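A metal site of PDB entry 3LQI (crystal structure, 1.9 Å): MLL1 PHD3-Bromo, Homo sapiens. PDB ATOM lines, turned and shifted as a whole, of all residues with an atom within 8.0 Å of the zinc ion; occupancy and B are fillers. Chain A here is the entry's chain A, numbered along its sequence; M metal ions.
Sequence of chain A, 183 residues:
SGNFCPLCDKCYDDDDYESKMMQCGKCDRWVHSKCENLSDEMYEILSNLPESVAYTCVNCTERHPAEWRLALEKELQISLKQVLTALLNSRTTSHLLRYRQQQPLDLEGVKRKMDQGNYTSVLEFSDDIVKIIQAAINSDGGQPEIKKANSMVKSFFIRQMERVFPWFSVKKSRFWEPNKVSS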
ATOM      1  N   PHE A   4     -18.338   2.200 -15.552  1.00  0.00           N
ATOM      2  CA  PHE A   4     -18.349   3.542 -14.979  1.00  0.00           C
ATOM      3  C   PHE A   4     -18.539   4.586 -16.079  1.00  0.00           C
ATOM      4  O   PHE A   4     -18.079   4.411 -17.196  1.00  0.00           O
ATOM      5  CB  PHE A   4     -17.020   3.814 -14.279  1.00  0.00           C
ATOM      6  CG  PHE A   4     -16.674   2.813 -13.218  1.00  0.00           C
ATOM      7  CD1 PHE A   4     -16.890   3.091 -11.880  1.00  0.00           C
ATOM      8  CD2 PHE A   4     -16.136   1.575 -13.573  1.00  0.00           C
ATOM      9  CE1 PHE A   4     -16.587   2.162 -10.886  1.00  0.00           C
ATOM     10  CE2 PHE A   4     -15.818   0.629 -12.587  1.00  0.00           C
ATOM     11  CZ  PHE A   4     -16.049   0.925 -11.240  1.00  0.00           C
ATOM     12  N   CYS A   5     -19.212   5.683 -15.736  1.00  0.00           N
ATOM     13  CA  CYS A   5     -19.402   6.754 -16.714  1.00  0.00           C
ATOM     14  C   CYS A   5     -18.007   7.284 -17.035  1.00  0.00           C
ATOM     15  O   CYS A   5     -17.244   7.610 -16.131  1.00  0.00           O
ATOM     16  CB  CYS A   5     -20.276   7.855 -16.114  1.00  0.00           C
ATOM     17  SG  CYS A   5     -20.290   9.364 -17.086  1.00  0.00           S
ATOM     18  N   PRO A   6     -17.643   7.387 -18.324  1.00  0.00           N
ATOM     19  CA  PRO A   6     -16.316   7.883 -18.684  1.00  0.00           C
ATOM     20  C   PRO A   6     -15.972   9.309 -18.246  1.00  0.00           C
ATOM     21  O   PRO A   6     -14.800   9.681 -18.240  1.00  0.00           O
ATOM     22  CB  PRO A   6     -16.264   7.714 -20.198  1.00  0.00           C
ATOM     23  CG  PRO A   6     -17.720   7.807 -20.615  1.00  0.00           C
ATOM     24  CD  PRO A   6     -18.412   6.998 -19.531  1.00  0.00           C
ATOM     25  N   LEU A   7     -16.970  10.103 -17.882  1.00  0.00           N
ATOM     26  CA  LEU A   7     -16.686  11.463 -17.445  1.00  0.00           C
ATOM     27  C   LEU A   7     -16.597  11.676 -15.949  1.00  0.00           C
ATOM     28  O   LEU A   7     -15.614  12.208 -15.458  1.00  0.00           O
ATOM     29  CB  LEU A   7     -17.707  12.444 -18.006  1.00  0.00           C
ATOM     30  CG  LEU A   7     -17.275  12.942 -19.373  1.00  0.00           C
ATOM     31  CD1 LEU A   7     -18.270  12.459 -20.403  1.00  0.00           C
ATOM     32  CD2 LEU A   7     -17.163  14.467 -19.373  1.00  0.00           C
ATOM     33  N   CYS A   8     -17.616  11.260 -15.200  1.00  0.00           N
ATOM     34  CA  CYS A   8     -17.609  11.460 -13.750  1.00  0.00           C
ATOM     35  C   CYS A   8     -17.126  10.237 -12.967  1.00  0.00           C
ATOM     36  O   CYS A   8     -16.865  10.327 -11.770  1.00  0.00           O
ATOM     37  CB  CYS A   8     -19.005  11.847 -13.266  1.00  0.00           C
ATOM     38  SG  CYS A   8     -20.207  10.500 -13.328  1.00  0.00           S
ATOM     39  N   ASP A   9     -17.020   9.110 -13.661  1.00  0.00           N
ATOM     40  CA  ASP A   9     -16.550   7.852 -13.076  1.00  0.00           C
ATOM     41  C   ASP A   9     -17.486   7.212 -12.047  1.00  0.00           C
ATOM     42  O   ASP A   9     -17.053   6.392 -11.238  1.00  0.00           O
ATOM     43  CB  ASP A   9     -15.152   8.035 -12.467  1.00  0.00           C
ATOM     44  CG  ASP A   9     -14.418   6.712 -12.278  1.00  0.00           C
ATOM     45  OD1 ASP A   9     -14.472   5.870 -13.196  1.00  0.00           O
ATOM     46  OD2 ASP A   9     -13.785   6.522 -11.220  1.00  0.00           O
ATOM     47  N   LYS A  10     -18.773   7.576 -12.058  1.00  0.00           N
ATOM     48  CA  LYS A  10     -19.709   6.944 -11.138  1.00  0.00           C
ATOM     49  C   LYS A  10     -20.076   5.602 -11.747  1.00  0.00           C
ATOM     50  O   LYS A  10     -20.180   5.480 -12.967  1.00  0.00           O
ATOM     51  CB  LYS A  10     -20.978   7.772 -10.961  1.00  0.00           C
ATOM     52  CG  LYS A  10     -20.843   8.962 -10.033  1.00  0.00           C
ATOM     53  CD  LYS A  10     -22.216   9.495  -9.657  1.00  0.00           C
ATOM     54  CE  LYS A  10     -22.141  10.933  -9.197  1.00  0.00           C
ATOM     55  NZ  LYS A  10     -21.638  11.788 -10.320  1.00  0.00           N
ATOM     56  N   CYS A  11     -20.255   4.584 -10.903  1.00  0.00           N
ATOM     57  CA  CYS A  11     -20.596   3.265 -11.416  1.00  0.00           C
ATOM     58  C   CYS A  11     -22.069   3.158 -11.747  1.00  0.00           C
ATOM     59  O   CYS A  11     -22.893   3.942 -11.261  1.00  0.00           O
ATOM     60  CB  CYS A  11     -20.213   2.184 -10.400  1.00  0.00           C
ATOM     61  SG  CYS A  11     -21.033   2.346  -8.800  1.00  0.00           S
ATOM     62  N   TYR A  12     -22.405   2.185 -12.584  1.00  0.00           N
ATOM     63  CA  TYR A  12     -23.779   1.921 -12.984  1.00  0.00           C
ATOM     64  C   TYR A  12     -23.936   0.454 -13.325  1.00  0.00           C
ATOM     65  O   TYR A  12     -22.972  -0.214 -13.701  1.00  0.00           O
ATOM     66  CB  TYR A  12     -24.168   2.777 -14.188  1.00  0.00           C
ATOM     67  CG  TYR A  12     -23.318   2.575 -15.440  1.00  0.00           C
ATOM     68  CD1 TYR A  12     -22.387   3.537 -15.829  1.00  0.00           C
ATOM     69  CD2 TYR A  12     -23.471   1.443 -16.237  1.00  0.00           C
ATOM     70  CE1 TYR A  12     -21.628   3.381 -16.994  1.00  0.00           C
ATOM     71  CE2 TYR A  12     -22.719   1.280 -17.412  1.00  0.00           C
ATOM     72  CZ  TYR A  12     -21.797   2.258 -17.777  1.00  0.00           C
ATOM     73  OH  TYR A  12     -21.056   2.110 -18.915  1.00  0.00           O
ATOM     74  N   LYS A  20     -30.696   8.663 -15.944  1.00  0.00           N
ATOM     75  CA  LYS A  20     -30.767   9.457 -17.155  1.00  0.00           C
ATOM     76  C   LYS A  20     -29.375   9.409 -17.769  1.00  0.00           C
ATOM     77  O   LYS A  20     -28.482  10.150 -17.359  1.00  0.00           O
ATOM     78  CB  LYS A  20     -31.187  10.895 -16.825  1.00  0.00           C
ATOM     79  CG  LYS A  20     -32.649  10.992 -16.374  1.00  0.00           C
ATOM     80  CD  LYS A  20     -33.185  12.407 -16.506  1.00  0.00           C
ATOM     81  CE  LYS A  20     -32.738  13.283 -15.354  1.00  0.00           C
ATOM     82  NZ  LYS A  20     -33.573  13.053 -14.133  1.00  0.00           N
ATOM     83  N   MET A  21     -29.209   8.509 -18.732  1.00  0.00           N
ATOM     84  CA  MET A  21     -27.934   8.314 -19.385  1.00  0.00           C
ATOM     85  C   MET A  21     -28.114   7.973 -20.861  1.00  0.00           C
ATOM     86  O   MET A  21     -29.181   7.531 -21.292  1.00  0.00           O
ATOM     87  CB  MET A  21     -27.154   7.170 -18.704  1.00  0.00           C
ATOM     88  CG  MET A  21     -27.000   7.309 -17.196  1.00  0.00           C
ATOM     89  SD  MET A  21     -26.016   5.969 -16.442  1.00  0.00           S
ATOM     90  CE  MET A  21     -24.345   6.537 -16.818  1.00  0.00           C
ATOM     91  N   TRP A  30     -22.044   4.067 -20.972  1.00  0.00           N
ATOM     92  CA  TRP A  30     -23.168   4.936 -20.683  1.00  0.00           C
ATOM     93  C   TRP A  30     -22.633   6.206 -20.050  1.00  0.00           C
ATOM     94  O   TRP A  30     -21.725   6.165 -19.216  1.00  0.00           O
ATOM     95  CB  TRP A  30     -24.168   4.268 -19.721  1.00  0.00           C
ATOM     96  CG  TRP A  30     -24.968   3.170 -20.354  1.00  0.00           C
ATOM     97  CD1 TRP A  30     -24.624   1.850 -20.450  1.00  0.00           C
ATOM     98  CD2 TRP A  30     -26.250   3.289 -20.983  1.00  0.00           C
ATOM     99  NE1 TRP A  30     -25.603   1.148 -21.087  1.00  0.00           N
ATOM    100  CE2 TRP A  30     -26.622   1.997 -21.424  1.00  0.00           C
ATOM    101  CE3 TRP A  30     -27.124   4.362 -21.197  1.00  0.00           C
ATOM    102  CZ2 TRP A  30     -27.830   1.758 -22.090  1.00  0.00           C
ATOM    103  CZ3 TRP A  30     -28.321   4.117 -21.855  1.00  0.00           C
ATOM    104  CH2 TRP A  30     -28.662   2.825 -22.298  1.00  0.00           C
ATOM    105  N   VAL A  31     -23.210   7.330 -20.437  1.00  0.00           N
ATOM    106  CA  VAL A  31     -22.793   8.630 -19.921  1.00  0.00           C
ATOM    107  C   VAL A  31     -24.008   9.376 -19.371  1.00  0.00           C
ATOM    108  O   VAL A  31     -25.043   9.433 -20.020  1.00  0.00           O
ATOM    109  CB  VAL A  31     -22.168   9.467 -21.063  1.00  0.00           C
ATOM    110  CG1 VAL A  31     -21.808  10.860 -20.570  1.00  0.00           C
ATOM    111  CG2 VAL A  31     -20.950   8.743 -21.602  1.00  0.00           C
ATOM    112  N   HIS A  32     -23.870   9.943 -18.175  1.00  0.00           N
ATOM    113  CA  HIS A  32     -24.967  10.699 -17.551  1.00  0.00           C
ATOM    114  C   HIS A  32     -25.360  11.919 -18.363  1.00  0.00           C
ATOM    115  O   HIS A  32     -24.518  12.599 -18.941  1.00  0.00           O
ATOM    116  CB  HIS A  32     -24.594  11.185 -16.147  1.00  0.00           C
ATOM    117  CG  HIS A  32     -24.340  10.099 -15.161  1.00  0.00           C
ATOM    118  ND1 HIS A  32     -23.076   9.652 -14.855  1.00  0.00           N
ATOM    119  CD2 HIS A  32     -25.188   9.337 -14.423  1.00  0.00           C
ATOM    120  CE1 HIS A  32     -23.146   8.670 -13.972  1.00  0.00           C
ATOM    121  NE2 HIS A  32     -24.432   8.460 -13.699  1.00  0.00           N
ATOM    122  N   SER A  33     -26.658  12.220 -18.358  1.00  0.00           N
ATOM    123  CA  SER A  33     -27.161  13.396 -19.050  1.00  0.00           C
ATOM    124  C   SER A  33     -26.448  14.621 -18.475  1.00  0.00           C
ATOM    125  O   SER A  33     -26.058  15.521 -19.209  1.00  0.00           O
ATOM    126  CB  SER A  33     -28.668  13.527 -18.820  1.00  0.00           C
ATOM    127  OG  SER A  33     -29.150  14.719 -19.426  1.00  0.00           O
ATOM    128  N   LYS A  34     -26.270  14.637 -17.152  1.00  0.00           N
ATOM    129  CA  LYS A  34     -25.605  15.759 -16.494  1.00  0.00           C
ATOM    130  C   LYS A  34     -24.153  15.909 -16.946  1.00  0.00           C
ATOM    131  O   LYS A  34     -23.613  17.011 -16.962  1.00  0.00           O
ATOM    132  CB  LYS A  34     -25.638  15.594 -14.978  1.00  0.00           C
ATOM    133  CG  LYS A  34     -24.809  14.425 -14.454  1.00  0.00           C
ATOM    134  CD  LYS A  34     -24.729  14.457 -12.933  1.00  0.00           C
ATOM    135  CE  LYS A  34     -23.803  13.369 -12.407  1.00  0.00           C
ATOM    136  NZ  LYS A  34     -22.376  13.623 -12.750  1.00  0.00           N
ATOM    137  N   CYS A  35     -23.514  14.801 -17.318  1.00  0.00           N
ATOM    138  CA  CYS A  35     -22.113  14.861 -17.736  1.00  0.00           C
ATOM    139  C   CYS A  35     -21.896  15.421 -19.136  1.00  0.00           C
ATOM    140  O   CYS A  35     -20.754  15.624 -19.559  1.00  0.00           O
ATOM    141  CB  CYS A  35     -21.465  13.485 -17.579  1.00  0.00           C
ATOM    142  SG  CYS A  35     -21.312  13.047 -15.824  1.00  0.00           S
ATOM    143  N   GLU A  36     -22.991  15.678 -19.847  1.00  0.00           N
ATOM    144  CA  GLU A  36     -22.936  16.284 -21.172  1.00  0.00           C
ATOM    145  C   GLU A  36     -23.603  17.660 -21.041  1.00  0.00           C
ATOM    146  O   GLU A  36     -23.891  18.320 -22.029  1.00  0.00           O
ATOM    147  CB  GLU A  36     -23.694  15.434 -22.212  1.00  0.00           C
ATOM    148  CG  GLU A  36     -22.954  14.153 -22.641  1.00  0.00           C
ATOM    149  CD  GLU A  36     -21.778  14.413 -23.580  1.00  0.00           C
ATOM    150  OE1 GLU A  36     -21.333  15.572 -23.697  1.00  0.00           O
ATOM    151  OE2 GLU A  36     -21.284  13.434 -24.187  1.00  0.00           O
HETATM  152 ZN    ZN M   1     -21.235  10.718 -15.462  1.00  0.00          ZN
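Four residues have an atom within 4 Å of the zinc ion: Cys 5, Cys 8, His 32 and Cys 35.
The zinc ion is bound by ND1 of His 32, SG of Cys 5, SG of Cys 35 and SG of Cys 8.
The zinc ion has four donor atoms within binding distance.
The backbone NH of Cys 5 sits at hydrogen-bond distance from the backbone carbonyl oxygen of Lys 10.
N of Leu 7 sits close to SG of Cys 5 (3.5 Å).
N of Lys 10 lies close to SG of Cys 8 (3.5 Å).
The side-chain amino group (NZ) of Lys 34 sits close to the side-chain sulfur (SG) of Cys 35.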
